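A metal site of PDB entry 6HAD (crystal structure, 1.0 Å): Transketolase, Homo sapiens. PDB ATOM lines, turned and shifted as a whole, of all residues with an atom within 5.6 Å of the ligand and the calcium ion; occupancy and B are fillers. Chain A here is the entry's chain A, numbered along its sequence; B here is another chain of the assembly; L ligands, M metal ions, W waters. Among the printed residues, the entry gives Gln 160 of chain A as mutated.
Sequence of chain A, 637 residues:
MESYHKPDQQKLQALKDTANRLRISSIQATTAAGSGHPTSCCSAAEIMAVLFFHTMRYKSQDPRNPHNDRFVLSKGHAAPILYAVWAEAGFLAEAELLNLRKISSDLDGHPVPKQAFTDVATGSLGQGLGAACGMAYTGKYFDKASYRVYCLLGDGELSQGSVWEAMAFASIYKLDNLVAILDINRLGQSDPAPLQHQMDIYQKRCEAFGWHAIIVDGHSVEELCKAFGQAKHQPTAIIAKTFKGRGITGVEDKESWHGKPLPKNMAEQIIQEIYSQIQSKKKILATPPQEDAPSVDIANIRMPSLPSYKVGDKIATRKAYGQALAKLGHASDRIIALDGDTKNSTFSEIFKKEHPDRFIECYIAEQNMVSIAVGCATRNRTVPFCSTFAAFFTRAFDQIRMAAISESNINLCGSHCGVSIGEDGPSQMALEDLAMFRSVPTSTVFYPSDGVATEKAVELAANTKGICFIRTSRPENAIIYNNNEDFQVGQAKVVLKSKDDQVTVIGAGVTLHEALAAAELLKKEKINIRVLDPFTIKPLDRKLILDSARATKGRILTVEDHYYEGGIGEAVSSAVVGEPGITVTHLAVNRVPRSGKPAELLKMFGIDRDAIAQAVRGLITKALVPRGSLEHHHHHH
Water W1 lies within hydrogen-bond range of O of Asp 183 (2.7 Å), O6 of the ligand (2.7 Å), N of Asp 155 (3.1 Å) and ND2 of Asn 185 (3.2 Å). Water W2 bridges a nitrogen (N3) of the ligand (3.2 Å) and the side-chain amide oxygen (OE1) of Gln 428 of chain B (3.4 Å). Water W5 lies within hydrogen-bond range of OE2 of Glu 366 of chain B (2.7 Å) and O of Gly 340 of chain B (2.7 Å). Water W4 lies within hydrogen-bond range of a ring nitrogen (NE2) of His 37 (2.8 Å), a ring nitrogen (NE2) of His 258 (3.0 Å) and a sulfur (S1) of the ligand (3.6 Å).
The calcium ion is bound by OD1 of Asp 155 (2.2 Å), O3 of the ligand (2.2 Å), O5 of the ligand (2.2 Å), O of Leu 187 (2.2 Å), OD1 of Asn 185 (2.2 Å) and water W1 (2.4 Å).
The side-chain hydroxyl (OG) of Ser 40 is in hydrogen-bond range of an oxygen (O7) of the ligand, at 2.6 Å. O6 of the ligand is in salt-bridge range of NZ of Lys 75. OE2 of Glu 366 of chain B sits at hydrogen-bond distance from N1 of the ligand, at 2.7 Å. A ring nitrogen (NE2) of His 77 is in hydrogen-bond range of an oxygen (O7) of the ligand (2.7 Å). The side-chain amino group (NZ) of Lys 244 lies within salt-bridge range of an oxygen (O7) of the ligand, 3.3 Å away. The backbone NH (N) of Gly 156 lies within hydrogen-bond range of an oxygen (O2) of the ligand (3.4 Å). N of Glu 157 is in hydrogen-bond range of O2 of the ligand. The backbone carbonyl oxygen (O) of Gly 123 lies within hydrogen-bond range of a nitrogen (N3) of the ligand (2.9 Å). N of Leu 125 sits at hydrogen-bond distance from N2 of the ligand (3.1 Å). A ring nitrogen (NE2) of His 258 lies close to a sulfur (S1) of the ligand (3.3 Å).
A nitrogen (N4) of the ligand sits close to the side-chain amide oxygen of Gln 189 (3.4 Å). Merely in contact with the ligand: Gln 160, Phe 392 of chain B, Ile 364 of chain B, Ser 124, Gly 154, Asp 341 of chain B, Arg 395 of chain B, Gln 428 of chain B, Gly 188 and Thr 342 of chain B. Hydrophobic or aromatic side chains within 4 Å of the ligand: His 77, Leu 125, His 258, Ile 364 of chain B and Phe 392 of chain B.
O of Asp 183 is in hydrogen-bond range of N of Asp 155 (3.4 Å). The backbone carbonyl oxygen (O) of Ser 40 sits at hydrogen-bond distance from the side-chain amino group (NZ) of Lys 75 (2.9 Å). The side-chain hydroxyl (OG) of Ser 43 sits at hydrogen-bond distance from the backbone carbonyl oxygen (O) of Ser 40 (3.4 Å). NZ of Lys 75 lies within salt-bridge range of OD2 of Asp 183 (2.7 Å). The side-chain amide nitrogen (NE2) of Gln 160 sits at hydrogen-bond distance from the side-chain carboxylate (OE1) of Glu 366 of chain B, 2.8 Å away. The side-chain amino group (NZ) of Lys 244 is in hydrogen-bond range of a ring nitrogen (ND1) of His 258, 2.8 Å away. The backbone NH (N) of Gly 154 is in hydrogen-bond range of the side-chain carboxylate (OE1) of Glu 157 (2.9 Å). OE1 of Gln 428 of chain B sits close to O of Gly 123 (2.9 Å).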
ATOM      1  N   HIS A  37      22.618  13.676  22.848  1.00  0.00           N
ATOM      2  CA  HIS A  37      22.157  13.401  21.500  1.00  0.00           C
ATOM      3  C   HIS A  37      20.766  12.744  21.510  1.00  0.00           C
ATOM      4  O   HIS A  37      20.606  11.633  21.000  1.00  0.00           O
ATOM      5  CB  HIS A  37      23.163  12.489  20.784  1.00  0.00           C
ATOM      6  CG  HIS A  37      24.522  13.078  20.655  1.00  0.00           C
ATOM      7  ND1 HIS A  37      25.371  13.200  21.729  1.00  0.00           N
ATOM      8  CD2 HIS A  37      25.188  13.516  19.569  1.00  0.00           C
ATOM      9  CE1 HIS A  37      26.498  13.741  21.303  1.00  0.00           C
ATOM     10  NE2 HIS A  37      26.415  13.953  20.005  1.00  0.00           N
ATOM     11  N   SER A  40      19.467  11.194  18.223  1.00  0.00           N
ATOM     12  CA  SER A  40      20.139   9.953  17.821  1.00  0.00           C
ATOM     13  C   SER A  40      19.637   8.776  18.648  1.00  0.00           C
ATOM     14  O   SER A  40      19.692   7.627  18.211  1.00  0.00           O
ATOM     15  CB  SER A  40      21.631  10.100  18.031  1.00  0.00           C
ATOM     16  OG  SER A  40      22.183  11.164  17.283  1.00  0.00           O
ATOM     17  N   SER A  43      15.731   7.779  17.157  1.00  0.00           N
ATOM     18  CA  SER A  43      15.610   6.969  15.948  1.00  0.00           C
ATOM     19  C   SER A  43      15.742   5.490  16.260  1.00  0.00           C
ATOM     20  O   SER A  43      15.247   4.663  15.498  1.00  0.00           O
ATOM     21  CB  SER A  43      16.587   7.353  14.834  1.00  0.00           C
ATOM     22  OG  SER A  43      17.934   7.348  15.274  1.00  0.00           O
ATOM     23  N   LYS A  75      27.180   3.224  17.444  1.00  0.00           N
ATOM     24  CA  LYS A  75      26.870   4.657  17.419  1.00  0.00           C
ATOM     25  C   LYS A  75      26.799   5.122  18.869  1.00  0.00           C
ATOM     26  O   LYS A  75      25.743   5.331  19.454  1.00  0.00           O
ATOM     27  CB  LYS A  75      25.600   4.965  16.598  1.00  0.00           C
ATOM     28  CG  LYS A  75      24.400   4.047  16.782  1.00  0.00           C
ATOM     29  CD  LYS A  75      23.159   4.602  16.104  1.00  0.00           C
ATOM     30  CE  LYS A  75      22.392   5.540  17.007  1.00  0.00           C
ATOM     31  NZ  LYS A  75      21.311   6.243  16.314  1.00  0.00           N
ATOM     32  N   HIS A  77      27.317   7.681  20.689  1.00  0.00           N
ATOM     33  CA  HIS A  77      26.719   8.923  21.171  1.00  0.00           C
ATOM     34  C   HIS A  77      25.231   8.720  21.506  1.00  0.00           C
ATOM     35  O   HIS A  77      24.616   9.599  22.119  1.00  0.00           O
ATOM     36  CB  HIS A  77      26.921  10.044  20.147  1.00  0.00           C
ATOM     37  CG  HIS A  77      26.465   9.680  18.783  1.00  0.00           C
ATOM     38  ND1 HIS A  77      27.127   8.763  17.973  1.00  0.00           N
ATOM     39  CD2 HIS A  77      25.367  10.069  18.110  1.00  0.00           C
ATOM     40  CE1 HIS A  77      26.446   8.649  16.848  1.00  0.00           C
ATOM     41  NE2 HIS A  77      25.374   9.427  16.911  1.00  0.00           N
ATOM     42  N   GLY A 123      32.487   5.540  20.489  1.00  0.00           N
ATOM     43  CA  GLY A 123      32.511   6.962  20.414  1.00  0.00           C
ATOM     44  C   GLY A 123      33.312   7.399  19.206  1.00  0.00           C
ATOM     45  O   GLY A 123      33.014   8.434  18.654  1.00  0.00           O
ATOM     46  N   SER A 124      34.320   6.622  18.817  1.00  0.00           N
ATOM     47  CA  SER A 124      34.947   6.801  17.526  1.00  0.00           C
ATOM     48  C   SER A 124      34.169   5.912  16.568  1.00  0.00           C
ATOM     49  O   SER A 124      34.212   4.677  16.664  1.00  0.00           O
ATOM     50  CB  SER A 124      36.406   6.423  17.540  1.00  0.00           C
ATOM     51  OG  SER A 124      36.820   6.429  16.190  1.00  0.00           O
ATOM     52  N   LEU A 125      33.432   6.524  15.665  1.00  0.00           N
ATOM     53  CA  LEU A 125      32.501   5.787  14.842  1.00  0.00           C
ATOM     54  C   LEU A 125      33.174   4.776  13.928  1.00  0.00           C
ATOM     55  O   LEU A 125      34.274   4.980  13.447  1.00  0.00           O
ATOM     56  CB  LEU A 125      31.694   6.776  13.999  1.00  0.00           C
ATOM     57  CG  LEU A 125      30.695   7.597  14.796  1.00  0.00           C
ATOM     58  CD1 LEU A 125      30.217   8.750  13.981  1.00  0.00           C
ATOM     59  CD2 LEU A 125      29.506   6.729  15.202  1.00  0.00           C
ATOM     60  N   GLY A 154      25.013   3.623  13.114  1.00  0.00           N
ATOM     61  CA  GLY A 154      24.383   4.721  12.395  1.00  0.00           C
ATOM     62  C   GLY A 154      24.617   4.655  10.903  1.00  0.00           C
ATOM     63  O   GLY A 154      25.453   3.890  10.426  1.00  0.00           O
ATOM     64  N   ASP A 155      23.888   5.475  10.141  1.00  0.00           N
ATOM     65  CA  ASP A 155      24.093   5.497   8.711  1.00  0.00           C
ATOM     66  C   ASP A 155      25.275   6.352   8.272  1.00  0.00           C
ATOM     67  O   ASP A 155      26.025   5.927   7.400  1.00  0.00           O
ATOM     68  CB  ASP A 155      22.810   5.801   7.891  1.00  0.00           C
ATOM     69  CG  ASP A 155      22.073   7.103   8.231  1.00  0.00           C
ATOM     70  OD1 ASP A 155      22.437   7.817   9.167  1.00  0.00           O
ATOM     71  OD2 ASP A 155      21.080   7.366   7.513  1.00  0.00           O
ATOM     72  N   GLY A 156      25.485   7.511   8.892  1.00  0.00           N
ATOM     73  CA  GLY A 156      26.704   8.263   8.641  1.00  0.00           C
ATOM     74  C   GLY A 156      27.939   7.403   8.904  1.00  0.00           C
ATOM     75  O   GLY A 156      28.932   7.422   8.166  1.00  0.00           O
ATOM     76  N   GLU A 157      27.866   6.647   9.979  1.00  0.00           N
ATOM     77  CA  GLU A 157      28.893   5.751  10.408  1.00  0.00           C
ATOM     78  C   GLU A 157      29.328   4.768   9.306  1.00  0.00           C
ATOM     79  O   GLU A 157      30.496   4.359   9.264  1.00  0.00           O
ATOM     80  CB  GLU A 157      28.380   4.978  11.640  1.00  0.00           C
ATOM     81  CG  GLU A 157      29.349   4.004  12.184  1.00  0.00           C
ATOM     82  CD  GLU A 157      28.971   3.469  13.576  1.00  0.00           C
ATOM     83  OE1 GLU A 157      27.760   3.407  13.948  1.00  0.00           O
ATOM     84  OE2 GLU A 157      29.897   3.054  14.284  1.00  0.00           O
ATOM     85  N   LEU A 158      28.415   4.385   8.421  1.00  0.00           N
ATOM     86  CA  LEU A 158      28.683   3.440   7.341  1.00  0.00           C
ATOM     87  C   LEU A 158      29.624   3.992   6.278  1.00  0.00           C
ATOM     88  O   LEU A 158      30.048   3.251   5.405  1.00  0.00           O
ATOM     89  CB  LEU A 158      27.382   2.954   6.708  1.00  0.00           C
ATOM     90  CG  LEU A 158      26.400   2.356   7.697  1.00  0.00           C
ATOM     91  CD1 LEU A 158      25.073   2.070   7.000  1.00  0.00           C
ATOM     92  CD2 LEU A 158      26.957   1.121   8.387  1.00  0.00           C
ATOM     93  N   GLN A 160      32.594   4.798   7.106  1.00  0.00           N
ATOM     94  CA  GLN A 160      33.911   4.347   7.564  1.00  0.00           C
ATOM     95  C   GLN A 160      34.307   3.035   6.932  1.00  0.00           C
ATOM     96  O   GLN A 160      33.577   2.026   7.006  1.00  0.00           O
ATOM     97  CB  GLN A 160      33.930   4.165   9.084  1.00  0.00           C
ATOM     98  CG  GLN A 160      33.897   5.461   9.867  1.00  0.00           C
ATOM     99  CD  GLN A 160      35.218   6.196   9.856  1.00  0.00           C
ATOM    100  OE1 GLN A 160      36.149   5.888   9.098  1.00  0.00           O
ATOM    101  NE2 GLN A 160      35.334   7.163  10.740  1.00  0.00           N
ATOM    102  N   ASP A 183      20.764   1.894  11.621  1.00  0.00           N
ATOM    103  CA  ASP A 183      19.786   2.934  11.924  1.00  0.00           C
ATOM    104  C   ASP A 183      19.842   3.953  10.803  1.00  0.00           C
ATOM    105  O   ASP A 183      20.586   4.932  10.865  1.00  0.00           O
ATOM    106  CB  ASP A 183      20.110   3.517  13.304  1.00  0.00           C
ATOM    107  CG  ASP A 183      19.108   4.553  13.787  1.00  0.00           C
ATOM    108  OD1 ASP A 183      18.195   4.923  13.026  1.00  0.00           O
ATOM    109  OD2 ASP A 183      19.269   5.023  14.947  1.00  0.00           O
ATOM    110  N   ASN A 185      18.591   6.707   9.551  1.00  0.00           N
ATOM    111  CA  ASN A 185      17.756   7.847   9.908  1.00  0.00           C
ATOM    112  C   ASN A 185      18.001   9.070   9.036  1.00  0.00           C
ATOM    113  O   ASN A 185      17.517  10.169   9.374  1.00  0.00           O
ATOM    114  CB  ASN A 185      17.854   8.175  11.397  1.00  0.00           C
ATOM    115  CG  ASN A 185      19.202   8.700  11.802  1.00  0.00           C
ATOM    116  OD1 ASN A 185      20.006   9.101  10.962  1.00  0.00           O
ATOM    117  ND2 ASN A 185      19.463   8.688  13.098  1.00  0.00           N
ATOM    118  N   ARG A 186      18.682   8.888   7.925  1.00  0.00           N
ATOM    119  CA  ARG A 186      18.804   9.855   6.826  1.00  0.00           C
ATOM    120  C   ARG A 186      19.873  10.916   7.038  1.00  0.00           C
ATOM    121  O   ARG A 186      20.414  11.409   6.064  1.00  0.00           O
ATOM    122  CB  ARG A 186      17.469  10.523   6.486  1.00  0.00           C
ATOM    123  CG  ARG A 186      17.433  11.104   5.084  1.00  0.00           C
ATOM    124  CD  ARG A 186      16.090  11.758   4.779  1.00  0.00           C
ATOM    125  NE  ARG A 186      15.755  12.891   5.651  1.00  0.00           N
ATOM    126  CZ  ARG A 186      16.178  14.135   5.488  1.00  0.00           C
ATOM    127  NH1 ARG A 186      15.773  15.086   6.324  1.00  0.00           N
ATOM    128  NH2 ARG A 186      17.008  14.418   4.492  1.00  0.00           N
ATOM    129  N   LEU A 187      20.118  11.287   8.294  1.00  0.00           N
ATOM    130  CA  LEU A 187      20.914  12.442   8.632  1.00  0.00           C
ATOM    131  C   LEU A 187      22.182  12.077   9.374  1.00  0.00           C
ATOM    132  O   LEU A 187      22.173  11.205  10.232  1.00  0.00           O
ATOM    133  CB  LEU A 187      20.111  13.420   9.485  1.00  0.00           C
ATOM    134  CG  LEU A 187      18.865  14.002   8.828  1.00  0.00           C
ATOM    135  CD1 LEU A 187      18.142  14.912   9.812  1.00  0.00           C
ATOM    136  CD2 LEU A 187      19.198  14.710   7.547  1.00  0.00           C
ATOM    137  N   GLY A 188      23.259  12.801   9.092  1.00  0.00           N
ATOM    138  CA  GLY A 188      24.476  12.727   9.877  1.00  0.00           C
ATOM    139  C   GLY A 188      24.518  13.888  10.857  1.00  0.00           C
ATOM    140  O   GLY A 188      23.475  14.317  11.372  1.00  0.00           O
ATOM    141  N   GLN A 189      25.721  14.387  11.133  1.00  0.00           N
ATOM    142  CA  GLN A 189      25.901  15.478  12.079  1.00  0.00           C
ATOM    143  C   GLN A 189      25.605  16.841  11.467  1.00  0.00           C
ATOM    144  O   GLN A 189      24.994  17.687  12.112  1.00  0.00           O
ATOM    145  CB  GLN A 189      27.330  15.451  12.621  1.00  0.00           C
ATOM    146  CG  GLN A 189      27.687  16.726  13.378  1.00  0.00           C
ATOM    147  CD  GLN A 189      28.936  16.631  14.205  1.00  0.00           C
ATOM    148  OE1 GLN A 189      29.275  15.570  14.742  1.00  0.00           O
ATOM    149  NE2 GLN A 189      29.648  17.737  14.323  1.00  0.00           N
ATOM    150  N   ALA A 193      23.147  12.064   5.469  1.00  0.00           N
ATOM    151  CA  ALA A 193      24.089  11.028   5.106  1.00  0.00           C
ATOM    152  C   ALA A 193      24.034  10.840   3.579  1.00  0.00           C
ATOM    153  O   ALA A 193      22.991  11.062   2.979  1.00  0.00           O
ATOM    154  CB  ALA A 193      23.767   9.728   5.834  1.00  0.00           C
ATOM    155  N   LYS A 244      15.321  10.546  12.328  1.00  0.00           N
ATOM    156  CA  LYS A 244      16.096  11.106  13.413  1.00  0.00           C
ATOM    157  C   LYS A 244      15.170  11.955  14.274  1.00  0.00           C
ATOM    158  O   LYS A 244      14.320  12.657  13.761  1.00  0.00           O
ATOM    159  CB  LYS A 244      17.296  11.867  12.863  1.00  0.00           C
ATOM    160  CG  LYS A 244      18.427  12.067  13.875  1.00  0.00           C
ATOM    161  CD  LYS A 244      19.736  12.439  13.194  1.00  0.00           C
ATOM    162  CE  LYS A 244      20.881  12.648  14.150  1.00  0.00           C
ATOM    163  NZ  LYS A 244      22.201  12.609  13.466  1.00  0.00           N
ATOM    164  N   HIS A 258      21.488  17.529  15.569  1.00  0.00           N
ATOM    165  CA  HIS A 258      22.420  16.506  15.989  1.00  0.00           C
ATOM    166  C   HIS A 258      23.189  17.002  17.220  1.00  0.00           C
ATOM    167  O   HIS A 258      23.800  18.070  17.197  1.00  0.00           O
ATOM    168  CB  HIS A 258      23.416  16.147  14.903  1.00  0.00           C
ATOM    169  CG  HIS A 258      24.372  15.091  15.333  1.00  0.00           C
ATOM    170  ND1 HIS A 258      24.091  13.748  15.227  1.00  0.00           N
ATOM    171  CD2 HIS A 258      25.592  15.190  15.906  1.00  0.00           C
ATOM    172  CE1 HIS A 258      25.108  13.076  15.725  1.00  0.00           C
ATOM    173  NE2 HIS A 258      26.030  13.922  16.143  1.00  0.00           N
ATOM    174  N   ASP A 398      43.614   4.599  15.743  1.00  0.00           N
ATOM    175  CA  ASP A 398      42.376   4.949  16.452  1.00  0.00           C
ATOM    176  C   ASP A 398      41.770   3.728  17.162  1.00  0.00           C
ATOM    177  O   ASP A 398      41.215   3.828  18.244  1.00  0.00           O
ATOM    178  CB  ASP A 398      41.411   5.591  15.464  1.00  0.00           C
ATOM    179  CG  ASP A 398      40.202   6.302  16.094  1.00  0.00           C
ATOM    180  OD1 ASP A 398      40.239   6.662  17.285  1.00  0.00           O
ATOM    181  OD2 ASP A 398      39.230   6.493  15.332  1.00  0.00           O
ATOM    182  N   GLY B 340      35.120  16.106   7.575  1.00  0.00           N
ATOM    183  CA  GLY B 340      34.471  14.807   7.687  1.00  0.00           C
ATOM    184  C   GLY B 340      33.195  14.849   8.518  1.00  0.00           C
ATOM    185  O   GLY B 340      33.159  14.278   9.599  1.00  0.00           O
ATOM    186  N   ASP B 341      32.165  15.513   8.007  1.00  0.00           N
ATOM    187  CA  ASP B 341      30.857  15.649   8.683  1.00  0.00           C
ATOM    188  C   ASP B 341      30.969  16.323  10.053  1.00  0.00           C
ATOM    189  O   ASP B 341      30.136  16.078  10.897  1.00  0.00           O
ATOM    190  CB  ASP B 341      30.096  14.329   8.790  1.00  0.00           C
ATOM    191  CG  ASP B 341      28.625  14.497   9.155  1.00  0.00           C
ATOM    192  OD1 ASP B 341      28.007  15.549   8.800  1.00  0.00           O
ATOM    193  OD2 ASP B 341      28.058  13.557   9.760  1.00  0.00           O
ATOM    194  N   THR B 342      31.973  17.179  10.221  1.00  0.00           N
ATOM    195  CA  THR B 342      32.168  17.914  11.474  1.00  0.00           C
ATOM    196  C   THR B 342      32.249  19.413  11.283  1.00  0.00           C
ATOM    197  O   THR B 342      32.676  20.123  12.181  1.00  0.00           O
ATOM    198  CB  THR B 342      33.381  17.386  12.299  1.00  0.00           C
ATOM    199  OG1 THR B 342      34.592  17.368  11.530  1.00  0.00           O
ATOM    200  CG2 THR B 342      33.126  15.971  12.772  1.00  0.00           C
ATOM    201  N   ILE B 364      32.081  10.719   6.969  1.00  0.00           N
ATOM    202  CA  ILE B 364      32.746  10.169   8.166  1.00  0.00           C
ATOM    203  C   ILE B 364      33.712   9.101   7.679  1.00  0.00           C
ATOM    204  O   ILE B 364      33.440   7.899   7.706  1.00  0.00           O
ATOM    205  CB  ILE B 364      31.732   9.664   9.201  1.00  0.00           C
ATOM    206  CG1 ILE B 364      30.704  10.745   9.538  1.00  0.00           C
ATOM    207  CG2 ILE B 364      32.439   9.168  10.432  1.00  0.00           C
ATOM    208  CD1 ILE B 364      29.566  10.279  10.460  1.00  0.00           C
ATOM    209  N   GLU B 366      37.839   9.589   7.656  1.00  0.00           N
ATOM    210  CA  GLU B 366      39.030  10.414   7.806  1.00  0.00           C
ATOM    211  C   GLU B 366      40.228   9.916   7.004  1.00  0.00           C
ATOM    212  O   GLU B 366      41.018  10.722   6.540  1.00  0.00           O
ATOM    213  CB  GLU B 366      39.416  10.564   9.270  1.00  0.00           C
ATOM    214  CG  GLU B 366      38.376  11.257  10.146  1.00  0.00           C
ATOM    215  CD  GLU B 366      37.245  10.365  10.632  1.00  0.00           C
ATOM    216  OE1 GLU B 366      37.331   9.128  10.512  1.00  0.00           O
ATOM    217  OE2 GLU B 366      36.268  10.944  11.157  1.00  0.00           O
ATOM    218  N   THR B 388      38.831  17.984  11.196  1.00  0.00           N
ATOM    219  CA  THR B 388      37.973  17.122  11.992  1.00  0.00           C
ATOM    220  C   THR B 388      38.371  17.338  13.449  1.00  0.00           C
ATOM    221  O   THR B 388      39.170  18.224  13.753  1.00  0.00           O
ATOM    222  CB  THR B 388      38.066  15.624  11.546  1.00  0.00           C
ATOM    223  OG1 THR B 388      37.218  14.832  12.386  1.00  0.00           O
ATOM    224  CG2 THR B 388      39.461  15.052  11.691  1.00  0.00           C
ATOM    225  N   PHE B 389      37.828  16.558  14.373  1.00  0.00           N
ATOM    226  CA  PHE B 389      38.353  16.540  15.731  1.00  0.00           C
ATOM    227  C   PHE B 389      39.766  15.942  15.705  1.00  0.00           C
ATOM    228  O   PHE B 389      40.002  14.941  15.030  1.00  0.00           O
ATOM    229  CB  PHE B 389      37.516  15.647  16.654  1.00  0.00           C
ATOM    230  CG  PHE B 389      36.168  16.186  17.024  1.00  0.00           C
ATOM    231  CD1 PHE B 389      35.456  17.005  16.210  1.00  0.00           C
ATOM    232  CD2 PHE B 389      35.640  15.841  18.255  1.00  0.00           C
ATOM    233  CE1 PHE B 389      34.198  17.459  16.612  1.00  0.00           C
ATOM    234  CE2 PHE B 389      34.403  16.271  18.663  1.00  0.00           C
ATOM    235  CZ  PHE B 389      33.677  17.082  17.838  1.00  0.00           C
ATOM    236  N   PHE B 392      40.326  12.194  15.897  1.00  0.00           N
ATOM    237  CA  PHE B 392      40.024  11.346  14.758  1.00  0.00           C
ATOM    238  C   PHE B 392      41.071  11.390  13.676  1.00  0.00           C
ATOM    239  O   PHE B 392      41.026  10.543  12.767  1.00  0.00           O
ATOM    240  CB  PHE B 392      38.593  11.574  14.241  1.00  0.00           C
ATOM    241  CG  PHE B 392      37.561  11.470  15.327  1.00  0.00           C
ATOM    242  CD1 PHE B 392      37.640  10.459  16.286  1.00  0.00           C
ATOM    243  CD2 PHE B 392      36.565  12.415  15.446  1.00  0.00           C
ATOM    244  CE1 PHE B 392      36.714  10.377  17.317  1.00  0.00           C
ATOM    245  CE2 PHE B 392      35.651  12.350  16.487  1.00  0.00           C
ATOM    246  CZ  PHE B 392      35.749  11.333  17.410  1.00  0.00           C
ATOM    247  N   ARG B 395      42.783   8.085  13.243  1.00  0.00           N
ATOM    248  CA  ARG B 395      42.187   7.140  12.291  1.00  0.00           C
ATOM    249  C   ARG B 395      42.915   7.176  10.938  1.00  0.00           C
ATOM    250  O   ARG B 395      42.765   6.238  10.142  1.00  0.00           O
ATOM    251  CB  ARG B 395      40.706   7.490  12.138  1.00  0.00           C
ATOM    252  CG  ARG B 395      39.852   6.462  11.390  1.00  0.00           C
ATOM    253  CD  ARG B 395      39.859   5.102  12.054  1.00  0.00           C
ATOM    254  NE  ARG B 395      38.672   4.359  11.714  1.00  0.00           N
ATOM    255  CZ  ARG B 395      37.515   4.527  12.360  1.00  0.00           C
ATOM    256  NH1 ARG B 395      37.411   5.395  13.363  1.00  0.00           N
ATOM    257  NH2 ARG B 395      36.442   3.865  11.970  1.00  0.00           N
ATOM    258  N   GLN B 428      36.392  11.382  22.388  1.00  0.00           N
ATOM    259  CA  GLN B 428      36.462  12.593  21.562  1.00  0.00           C
ATOM    260  C   GLN B 428      37.677  13.459  21.891  1.00  0.00           C
ATOM    261  O   GLN B 428      37.862  14.474  21.236  1.00  0.00           O
ATOM    262  CB  GLN B 428      35.175  13.438  21.751  1.00  0.00           C
ATOM    263  CG  GLN B 428      33.830  12.620  21.758  1.00  0.00           C
ATOM    264  CD  GLN B 428      33.536  11.863  20.486  1.00  0.00           C
ATOM    265  OE1 GLN B 428      33.491  10.614  20.477  1.00  0.00           O
ATOM    266  NE2 GLN B 428      33.368  12.582  19.400  1.00  0.00           N
HETATM  267  N1  LIG L   1      34.623  10.654  13.225  1.00  0.00           N
HETATM  268  C1  LIG L   1      34.681   9.602  14.034  1.00  0.00           C
HETATM  269  C2  LIG L   1      35.659   8.521  13.706  1.00  0.00           C
HETATM  270  N2  LIG L   1      33.918   9.504  15.117  1.00  0.00           N
HETATM  271  C3  LIG L   1      33.100  10.499  15.446  1.00  0.00           C
HETATM  272  N3  LIG L   1      32.437  10.369  16.582  1.00  0.00           N
HETATM  273  C4  LIG L   1      32.955  11.672  14.579  1.00  0.00           C
HETATM  274  C5  LIG L   1      33.776  11.666  13.460  1.00  0.00           C
HETATM  275  C6  LIG L   1      32.055  12.871  14.941  1.00  0.00           C
HETATM  276  N4  LIG L   1      30.657  12.475  14.994  1.00  0.00           N
HETATM  277  C7  LIG L   1      29.979  12.131  16.117  1.00  0.00           C
HETATM  278  S1  LIG L   1      28.365  11.596  15.878  1.00  0.00           S
HETATM  279  C8  LIG L   1      28.560  11.995  14.172  1.00  0.00           C
HETATM  280  C9  LIG L   1      29.874  12.491  13.889  1.00  0.00           C
HETATM  281  C10 LIG L   1      30.338  12.901  12.543  1.00  0.00           C
HETATM  282  C11 LIG L   1      27.447  11.809  13.229  1.00  0.00           C
HETATM  283  C12 LIG L   1      27.013  10.361  13.302  1.00  0.00           C
HETATM  284  O1  LIG L   1      25.934  10.181  12.416  1.00  0.00           O
HETATM  285  P1  LIG L   1      25.276   8.738  12.248  1.00  0.00           P
HETATM  286  O2  LIG L   1      26.298   7.669  12.161  1.00  0.00           O
HETATM  287  O3  LIG L   1      24.365   8.901  11.100  1.00  0.00           O
HETATM  288  O4  LIG L   1      24.454   8.553  13.622  1.00  0.00           O
HETATM  289  P2  LIG L   1      23.027   9.142  14.118  1.00  0.00           P
HETATM  290  O5  LIG L   1      22.365   9.844  12.955  1.00  0.00           O
HETATM  291  O6  LIG L   1      22.257   7.922  14.521  1.00  0.00           O
HETATM  292  O7  LIG L   1      23.394  10.079  15.243  1.00  0.00           O
HETATM  293 CA    CA M   1      22.212   9.106  10.893  1.00  0.00          CA
HETATM  294  O   HOH W   1      21.941   7.006  11.963  1.00  0.00           O
HETATM  295  O   HOH W   2      30.457  10.827  19.051  1.00  0.00           O
HETATM  296  O   HOH W   3      30.507  15.382  17.093  1.00  0.00           O
HETATM  297  O   HOH W   4      28.300  14.491  18.001  1.00  0.00           O
HETATM  298  O   HOH W   5      35.355  13.448  11.029  1.00  0.00           O
